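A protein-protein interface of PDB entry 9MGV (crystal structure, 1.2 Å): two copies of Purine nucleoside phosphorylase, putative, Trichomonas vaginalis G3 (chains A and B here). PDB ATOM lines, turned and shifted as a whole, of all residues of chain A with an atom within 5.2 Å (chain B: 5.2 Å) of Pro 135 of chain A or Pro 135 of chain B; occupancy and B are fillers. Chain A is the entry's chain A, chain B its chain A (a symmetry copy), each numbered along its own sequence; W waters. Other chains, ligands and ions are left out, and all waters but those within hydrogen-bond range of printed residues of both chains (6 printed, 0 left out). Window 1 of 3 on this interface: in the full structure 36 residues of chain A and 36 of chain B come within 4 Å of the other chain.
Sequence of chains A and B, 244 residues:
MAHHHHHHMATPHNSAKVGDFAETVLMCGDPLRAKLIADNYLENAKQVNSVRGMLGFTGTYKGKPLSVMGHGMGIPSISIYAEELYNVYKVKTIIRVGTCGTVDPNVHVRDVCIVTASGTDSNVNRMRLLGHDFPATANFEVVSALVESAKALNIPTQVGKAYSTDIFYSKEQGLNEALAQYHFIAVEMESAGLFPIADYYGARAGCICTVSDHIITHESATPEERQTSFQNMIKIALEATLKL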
ATOM      1  N   ALA A 117     -11.046  23.599 -32.142  1.00  0.00           N
ATOM      2  CA  ALA A 117     -10.149  24.568 -31.520  1.00  0.00           C
ATOM      3  C   ALA A 117      -9.077  24.875 -32.549  1.00  0.00           C
ATOM      4  O   ALA A 117      -8.855  24.085 -33.467  1.00  0.00           O
ATOM      5  CB  ALA A 117      -9.517  24.019 -30.238  1.00  0.00           C
ATOM      6  N   SER A 118      -8.387  25.999 -32.382  1.00  0.00           N
ATOM      7  CA  SER A 118      -7.378  26.414 -33.343  1.00  0.00           C
ATOM      8  C   SER A 118      -6.123  26.897 -32.650  1.00  0.00           C
ATOM      9  O   SER A 118      -6.191  27.784 -31.805  1.00  0.00           O
ATOM     10  CB  SER A 118      -7.932  27.555 -34.192  1.00  0.00           C
ATOM     11  OG  SER A 118      -9.139  27.123 -34.748  1.00  0.00           O
ATOM     12  N   GLY A 119      -4.983  26.341 -33.034  1.00  0.00           N
ATOM     13  CA  GLY A 119      -3.698  26.840 -32.602  1.00  0.00           C
ATOM     14  C   GLY A 119      -3.318  28.079 -33.385  1.00  0.00           C
ATOM     15  O   GLY A 119      -4.006  28.492 -34.324  1.00  0.00           O
ATOM     16  N   ASP A 133      -1.076  29.846 -22.110  1.00  0.00           N
ATOM     17  CA  ASP A 133      -1.727  29.192 -23.242  1.00  0.00           C
ATOM     18  C   ASP A 133      -3.244  29.262 -23.067  1.00  0.00           C
ATOM     19  O   ASP A 133      -3.801  28.667 -22.134  1.00  0.00           O
ATOM     20  CB  ASP A 133      -1.345  27.718 -23.384  1.00  0.00           C
ATOM     21  CG  ASP A 133       0.068  27.487 -23.878  1.00  0.00           C
ATOM     22  OD1 ASP A 133       0.863  28.426 -23.911  1.00  0.00           O
ATOM     23  OD2 ASP A 133       0.394  26.322 -24.216  1.00  0.00           O
ATOM     24  N   PHE A 134      -3.896  29.988 -23.971  1.00  0.00           N
ATOM     25  CA  PHE A 134      -5.337  30.200 -24.001  1.00  0.00           C
ATOM     26  C   PHE A 134      -5.826  29.505 -25.259  1.00  0.00           C
ATOM     27  O   PHE A 134      -5.587  30.007 -26.359  1.00  0.00           O
ATOM     28  CB  PHE A 134      -5.566  31.712 -24.080  1.00  0.00           C
ATOM     29  CG  PHE A 134      -7.013  32.179 -24.150  1.00  0.00           C
ATOM     30  CD1 PHE A 134      -8.086  31.345 -24.391  1.00  0.00           C
ATOM     31  CD2 PHE A 134      -7.269  33.526 -23.990  1.00  0.00           C
ATOM     32  CE1 PHE A 134      -9.379  31.861 -24.480  1.00  0.00           C
ATOM     33  CE2 PHE A 134      -8.541  34.034 -24.081  1.00  0.00           C
ATOM     34  CZ  PHE A 134      -9.601  33.190 -24.322  1.00  0.00           C
ATOM     35  N   PRO A 135      -6.488  28.355 -25.164  1.00  0.00           N
ATOM     36  CA  PRO A 135      -6.931  27.664 -26.383  1.00  0.00           C
ATOM     37  C   PRO A 135      -8.084  28.421 -27.011  1.00  0.00           C
ATOM     38  O   PRO A 135      -9.090  28.696 -26.356  1.00  0.00           O
ATOM     39  CB  PRO A 135      -7.381  26.295 -25.872  1.00  0.00           C
ATOM     40  CG  PRO A 135      -7.840  26.568 -24.463  1.00  0.00           C
ATOM     41  CD  PRO A 135      -6.908  27.644 -23.947  1.00  0.00           C
ATOM     42  N   ALA A 136      -7.944  28.723 -28.295  1.00  0.00           N
ATOM     43  CA  ALA A 136      -9.036  29.294 -29.076  1.00  0.00           C
ATOM     44  C   ALA A 136      -9.988  28.148 -29.378  1.00  0.00           C
ATOM     45  O   ALA A 136      -9.657  27.266 -30.172  1.00  0.00           O
ATOM     46  CB  ALA A 136      -8.476  29.895 -30.359  1.00  0.00           C
ATOM     47  N   THR A 137     -11.144  28.138 -28.722  1.00  0.00           N
ATOM     48  CA  THR A 137     -12.004  26.959 -28.649  1.00  0.00           C
ATOM     49  C   THR A 137     -13.388  27.297 -29.189  1.00  0.00           C
ATOM     50  O   THR A 137     -13.997  28.280 -28.765  1.00  0.00           O
ATOM     51  CB  THR A 137     -12.107  26.466 -27.189  1.00  0.00           C
ATOM     52  OG1 THR A 137     -10.794  26.333 -26.639  1.00  0.00           O
ATOM     53  CG2 THR A 137     -12.797  25.138 -27.112  1.00  0.00           C
ATOM     54  N   LYS A 161      -8.764  19.888 -34.865  1.00  0.00           N
ATOM     55  CA  LYS A 161      -8.055  21.141 -34.655  1.00  0.00           C
ATOM     56  C   LYS A 161      -7.652  21.819 -35.959  1.00  0.00           C
ATOM     57  O   LYS A 161      -7.195  21.174 -36.899  1.00  0.00           O
ATOM     58  CB  LYS A 161      -6.771  20.890 -33.865  1.00  0.00           C
ATOM     59  CG  LYS A 161      -6.944  20.337 -32.460  1.00  0.00           C
ATOM     60  CD  LYS A 161      -5.611  20.149 -31.753  1.00  0.00           C
ATOM     61  CE  LYS A 161      -4.643  19.222 -32.471  1.00  0.00           C
ATOM     62  NZ  LYS A 161      -5.161  17.844 -32.568  1.00  0.00           N
ATOM     63  N   ALA A 162      -7.753  23.145 -35.975  1.00  0.00           N
ATOM     64  CA  ALA A 162      -7.147  23.979 -36.997  1.00  0.00           C
ATOM     65  C   ALA A 162      -5.892  24.645 -36.452  1.00  0.00           C
ATOM     66  O   ALA A 162      -5.626  24.644 -35.248  1.00  0.00           O
ATOM     67  CB  ALA A 162      -8.131  25.047 -37.469  1.00  0.00           C
ATOM     68  N   PHE A 184      -3.426  18.121 -36.611  1.00  0.00           N
ATOM     69  CA  PHE A 184      -4.120  19.326 -37.029  1.00  0.00           C
ATOM     70  C   PHE A 184      -4.681  19.078 -38.416  1.00  0.00           C
ATOM     71  O   PHE A 184      -3.939  18.701 -39.330  1.00  0.00           O
ATOM     72  CB  PHE A 184      -3.159  20.516 -37.040  1.00  0.00           C
ATOM     73  CG  PHE A 184      -2.823  21.025 -35.672  1.00  0.00           C
ATOM     74  CD1 PHE A 184      -1.845  20.421 -34.883  1.00  0.00           C
ATOM     75  CD2 PHE A 184      -3.508  22.111 -35.152  1.00  0.00           C
ATOM     76  CE1 PHE A 184      -1.565  20.893 -33.619  1.00  0.00           C
ATOM     77  CE2 PHE A 184      -3.218  22.592 -33.890  1.00  0.00           C
ATOM     78  CZ  PHE A 184      -2.250  21.978 -33.126  1.00  0.00           C
ATOM     79  N   ASP A 199     -15.641  34.556 -26.597  1.00  0.00           N
ATOM     80  CA  ASP A 199     -15.587  34.312 -25.160  1.00  0.00           C
ATOM     81  C   ASP A 199     -15.703  35.619 -24.376  1.00  0.00           C
ATOM     82  O   ASP A 199     -16.445  35.700 -23.390  1.00  0.00           O
ATOM     83  CB  ASP A 199     -14.274  33.640 -24.765  1.00  0.00           C
ATOM     84  CG  ASP A 199     -14.129  32.212 -25.225  1.00  0.00           C
ATOM     85  OD1 ASP A 199     -15.127  31.538 -25.531  1.00  0.00           O
ATOM     86  OD2 ASP A 199     -12.963  31.743 -25.221  1.00  0.00           O
ATOM     87  N   ALA B 117     -11.581  21.959 -24.143  1.00  0.00           N
ATOM     88  CA  ALA B 117     -10.170  22.272 -24.347  1.00  0.00           C
ATOM     89  C   ALA B 117      -9.666  22.841 -23.034  1.00  0.00           C
ATOM     90  O   ALA B 117     -10.459  23.313 -22.219  1.00  0.00           O
ATOM     91  CB  ALA B 117      -9.968  23.284 -25.479  1.00  0.00           C
ATOM     92  N   SER B 118      -8.351  22.829 -22.839  1.00  0.00           N
ATOM     93  CA  SER B 118      -7.770  23.297 -21.591  1.00  0.00           C
ATOM     94  C   SER B 118      -6.567  24.180 -21.839  1.00  0.00           C
ATOM     95  O   SER B 118      -5.638  23.770 -22.529  1.00  0.00           O
ATOM     96  CB  SER B 118      -7.327  22.095 -20.761  1.00  0.00           C
ATOM     97  OG  SER B 118      -8.427  21.245 -20.622  1.00  0.00           O
ATOM     98  N   GLY B 119      -6.571  25.366 -21.250  1.00  0.00           N
ATOM     99  CA  GLY B 119      -5.409  26.226 -21.240  1.00  0.00           C
ATOM    100  C   GLY B 119      -4.407  25.754 -20.207  1.00  0.00           C
ATOM    101  O   GLY B 119      -4.656  24.821 -19.438  1.00  0.00           O
ATOM    102  N   ASP B 133       1.195  28.344 -30.066  1.00  0.00           N
ATOM    103  CA  ASP B 133       0.029  27.989 -29.262  1.00  0.00           C
ATOM    104  C   ASP B 133      -0.611  26.721 -29.827  1.00  0.00           C
ATOM    105  O   ASP B 133      -1.127  26.720 -30.953  1.00  0.00           O
ATOM    106  CB  ASP B 133      -1.042  29.080 -29.244  1.00  0.00           C
ATOM    107  CG  ASP B 133      -0.673  30.301 -28.428  1.00  0.00           C
ATOM    108  OD1 ASP B 133       0.487  30.447 -28.042  1.00  0.00           O
ATOM    109  OD2 ASP B 133      -1.568  31.149 -28.193  1.00  0.00           O
ATOM    110  N   PHE B 134      -0.574  25.653 -29.033  1.00  0.00           N
ATOM    111  CA  PHE B 134      -1.115  24.340 -29.362  1.00  0.00           C
ATOM    112  C   PHE B 134      -2.270  24.123 -28.401  1.00  0.00           C
ATOM    113  O   PHE B 134      -2.033  23.885 -27.215  1.00  0.00           O
ATOM    114  CB  PHE B 134       0.003  23.322 -29.122  1.00  0.00           C
ATOM    115  CG  PHE B 134      -0.340  21.862 -29.375  1.00  0.00           C
ATOM    116  CD1 PHE B 134      -1.623  21.387 -29.560  1.00  0.00           C
ATOM    117  CD2 PHE B 134       0.694  20.946 -29.395  1.00  0.00           C
ATOM    118  CE1 PHE B 134      -1.854  20.024 -29.746  1.00  0.00           C
ATOM    119  CE2 PHE B 134       0.465  19.604 -29.575  1.00  0.00           C
ATOM    120  CZ  PHE B 134      -0.820  19.146 -29.758  1.00  0.00           C
ATOM    121  N   PRO B 135      -3.522  24.210 -28.842  1.00  0.00           N
ATOM    122  CA  PRO B 135      -4.641  24.034 -27.905  1.00  0.00           C
ATOM    123  C   PRO B 135      -4.749  22.576 -27.504  1.00  0.00           C
ATOM    124  O   PRO B 135      -4.839  21.693 -28.357  1.00  0.00           O
ATOM    125  CB  PRO B 135      -5.857  24.477 -28.716  1.00  0.00           C
ATOM    126  CG  PRO B 135      -5.478  24.160 -30.140  1.00  0.00           C
ATOM    127  CD  PRO B 135      -3.990  24.428 -30.219  1.00  0.00           C
ATOM    128  N   ALA B 136      -4.776  22.336 -26.200  1.00  0.00           N
ATOM    129  CA  ALA B 136      -5.050  21.007 -25.666  1.00  0.00           C
ATOM    130  C   ALA B 136      -6.549  20.792 -25.807  1.00  0.00           C
ATOM    131  O   ALA B 136      -7.331  21.424 -25.094  1.00  0.00           O
ATOM    132  CB  ALA B 136      -4.623  20.954 -24.205  1.00  0.00           C
ATOM    133  N   THR B 137      -6.949  19.938 -26.743  1.00  0.00           N
ATOM    134  CA  THR B 137      -8.328  19.874 -27.221  1.00  0.00           C
ATOM    135  C   THR B 137      -8.873  18.464 -27.029  1.00  0.00           C
ATOM    136  O   THR B 137      -8.244  17.493 -27.450  1.00  0.00           O
ATOM    137  CB  THR B 137      -8.393  20.273 -28.711  1.00  0.00           C
ATOM    138  OG1 THR B 137      -7.710  21.515 -28.901  1.00  0.00           O
ATOM    139  CG2 THR B 137      -9.811  20.431 -29.169  1.00  0.00           C
ATOM    140  N   LYS B 161     -14.267  25.446 -21.493  1.00  0.00           N
ATOM    141  CA  LYS B 161     -12.824  25.388 -21.314  1.00  0.00           C
ATOM    142  C   LYS B 161     -12.415  25.160 -19.863  1.00  0.00           C
ATOM    143  O   LYS B 161     -12.978  25.747 -18.942  1.00  0.00           O
ATOM    144  CB  LYS B 161     -12.187  26.705 -21.757  1.00  0.00           C
ATOM    145  CG  LYS B 161     -12.353  27.071 -23.223  1.00  0.00           C
ATOM    146  CD  LYS B 161     -11.662  28.382 -23.565  1.00  0.00           C
ATOM    147  CE  LYS B 161     -12.148  29.577 -22.759  1.00  0.00           C
ATOM    148  NZ  LYS B 161     -13.570  29.878 -23.013  1.00  0.00           N
ATOM    149  N   ALA B 162     -11.371  24.358 -19.677  1.00  0.00           N
ATOM    150  CA  ALA B 162     -10.658  24.257 -18.416  1.00  0.00           C
ATOM    151  C   ALA B 162      -9.343  25.018 -18.497  1.00  0.00           C
ATOM    152  O   ALA B 162      -8.888  25.419 -19.571  1.00  0.00           O
ATOM    153  CB  ALA B 162     -10.384  22.795 -18.073  1.00  0.00           C
ATOM    154  N   PHE B 184     -13.577  30.560 -18.658  1.00  0.00           N
ATOM    155  CA  PHE B 184     -13.032  29.272 -18.267  1.00  0.00           C
ATOM    156  C   PHE B 184     -13.887  28.734 -17.135  1.00  0.00           C
ATOM    157  O   PHE B 184     -14.080  29.416 -16.122  1.00  0.00           O
ATOM    158  CB  PHE B 184     -11.578  29.424 -17.820  1.00  0.00           C
ATOM    159  CG  PHE B 184     -10.622  29.631 -18.954  1.00  0.00           C
ATOM    160  CD1 PHE B 184     -10.430  30.886 -19.531  1.00  0.00           C
ATOM    161  CD2 PHE B 184      -9.919  28.556 -19.470  1.00  0.00           C
ATOM    162  CE1 PHE B 184      -9.560  31.052 -20.588  1.00  0.00           C
ATOM    163  CE2 PHE B 184      -9.039  28.725 -20.521  1.00  0.00           C
ATOM    164  CZ  PHE B 184      -8.866  29.972 -21.079  1.00  0.00           C
ATOM    165  N   ASP B 199      -3.271  13.066 -29.017  1.00  0.00           N
ATOM    166  CA  ASP B 199      -3.059  13.457 -30.405  1.00  0.00           C
ATOM    167  C   ASP B 199      -1.822  12.773 -30.987  1.00  0.00           C
ATOM    168  O   ASP B 199      -1.854  12.261 -32.113  1.00  0.00           O
ATOM    169  CB  ASP B 199      -2.864  14.967 -30.528  1.00  0.00           C
ATOM    170  CG  ASP B 199      -4.099  15.789 -30.264  1.00  0.00           C
ATOM    171  OD1 ASP B 199      -5.230  15.281 -30.344  1.00  0.00           O
ATOM    172  OD2 ASP B 199      -3.913  17.009 -30.025  1.00  0.00           O
HETATM  173  O   HOH W   1      -1.517  24.362 -24.576  1.00  0.00           O
HETATM  174  O   HOH W   2      -7.155  17.116 -30.024  1.00  0.00           O
HETATM  175  O   HOH W   3       1.161  25.734 -26.828  1.00  0.00           O
HETATM  176  O   HOH W   4     -14.467  29.000 -26.079  1.00  0.00           O
HETATM  177  O   HOH W   5      -2.382  31.711 -25.590  1.00  0.00           O
HETATM  178  O   HOH W   6      -4.228  30.572 -28.659  1.00  0.00           O
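O of Pro 135 of chain A is in hydrogen-bond range of OG1 of Thr 137 of chain A, 2.9 Å away.
O of Ala 136 of chain B lies within hydrogen-bond range of N of Ser 118 of chain B (2.8 Å).
N of Ala 162 of chain B is in hydrogen-bond range of O of Ala 117 of chain B (2.9 Å).
N of Gly 119 of chain B lies within hydrogen-bond range of O of Ala 162 of chain B, 2.9 Å away.
The backbone NH (N) of Ser 118 of chain A lies within hydrogen-bond range of the backbone carbonyl oxygen (O) of Ala 136 of chain A.
The backbone carbonyl oxygen of Pro 135 of chain B is in hydrogen-bond range of the side-chain hydroxyl of Thr 137 of chain B (2.9 Å).
Ser 118 of chain A touches Pro 135 of chain B, and with the chains exchanged Pro 135 of chain A touches Ser 118 of chain B.
Gly 119 of chain A touches Pro 135 of chain B, and with the chains exchanged Pro 135 of chain A touches Gly 119 of chain B.
Pro 135 of chain A touches Lys 161 of chain B, and with the chains exchanged Lys 161 of chain A touches Pro 135 of chain B.
Thr 137 of chain A touches Lys 161 of chain B, and with the chains exchanged Lys 161 of chain A touches Thr 137 of chain B.
Of the 21 pairs that touch across the chains among the printed residues, 21 have their exchanged pair printed and touching as well.
Water W2 lies within hydrogen-bond range of the side-chain carboxylate (OD1) of Asp 199 of chain B (2.7 Å), the backbone carbonyl oxygen (O) of Thr 137 of chain B (2.8 Å) and the side-chain amino group (NZ) of Lys 161 of chain A (3.3 Å).
Water W4 lies within hydrogen-bond range of the side-chain carboxylate (OD1) of Asp 199 of chain A (2.7 Å), the backbone carbonyl oxygen (O) of Thr 137 of chain A (2.8 Å) and the side-chain amino group (NZ) of Lys 161 of chain B (3.3 Å).
Water W1 bridges O of Phe 134 of chain B (2.7 Å) and OD2 of Asp 133 of chain A (2.8 Å).
Water W6 lies within hydrogen-bond range of O of Phe 134 of chain A (2.7 Å) and OD2 of Asp 133 of chain B (2.8 Å).
Water W5 bridges the side-chain carboxylate (OD2) of Asp 133 of chain B and the backbone NH (N) of Phe 134 of chain A.
Water W3 bridges OD2 of Asp 133 of chain A and N of Phe 134 of chain B.
CB of Ala 117 of chain A touches CB of Pro 135 of chain B, at 3.99 Å.
Ala 117 of chain A touches Thr 137 of chain B (CB to OG1, 3.4 Å).
Ser 118 of chain A touches Pro 135 of chain B (C to CG, 3.8 Å).
Asp 133 of chain B touches Gly 119 of chain A.
CE1 of Phe 134 of chain A touches CE of Lys 161 of chain B, 3.98 Å away.
Ser 118 of chain B touches Pro 135 of chain A (C to CG, 3.8 Å).
Gly 119 of chain B touches Pro 135 of chain A (CA to CD, 3.4 Å).
Pro 135 of chain A touches Lys 161 of chain B.
O of Pro 135 of chain B touches CD of Lys 161 of chain A, 3.8 Å away.
CZ of Phe 184 of chain A touches CD1 of Phe 134 of chain B, 3.7 Å away.
Printed residues of chain B that touch a printed residue of chain A: Ala 117, Ser 118, Gly 119, Asp 133, Phe 134, Pro 135, Thr 137, Lys 161, Phe 184 and Asp 199.
Printed residues of chain A that touch a printed residue of chain B: Ala 117, Ser 118, Gly 119, Asp 133, Phe 134, Pro 135, Thr 137, Lys 161, Phe 184 and Asp 199.
Hydrophobic or aromatic side chains of chain A within 4 Å of the printed part of chain B: Ala 117, Phe 134, Pro 135 and Phe 184.
Among the printed residues, Asp or Glu carboxylates within 4 Å of a Lys or Arg side-chain nitrogen of the other chain: Lys 161 of chain A with Asp 199 of chain B (3.0 Å) and Asp 199 of chain A with Lys 161 of chain B (3.0 Å).
Of the printed residues of chain B, Pro 135 of chain A touches Ala 117 (3.99 Å), Ser 118 (3.8 Å), Gly 119 (3.4 Å), Pro 135 (3.7 Å) and Lys 161 (3.8 Å).
Printed residues of chain A within 4 Å of Pro 135 of chain B: Ala 117 (3.99 Å), Ser 118 (3.8 Å), Gly 119 (3.4 Å), Pro 135 (3.7 Å) and Lys 161 (3.8 Å).
Printed residues of chain A within 4 Å of Phe 184 of chain B: Phe 134 (3.7 Å).
Of the printed residues of chain B, Lys 161 of chain A touches Phe 134 (3.98 Å), Pro 135 (3.8 Å), Thr 137 (3.8 Å) and Asp 199 (3.0 Å).
The nearest printed residue of chain B that does not touch Pro 135 of chain A is Phe 184 of chain B (4.2 Å).
The side-chain amino group (NZ) of Lys 161 of chain A is in salt-bridge range of the side-chain carboxylate (OD2) of Asp 199 of chain B, 3.0 Å away.
NZ of Lys 161 of chain B lies within salt-bridge range of OD2 of Asp 199 of chain A (3.0 Å).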
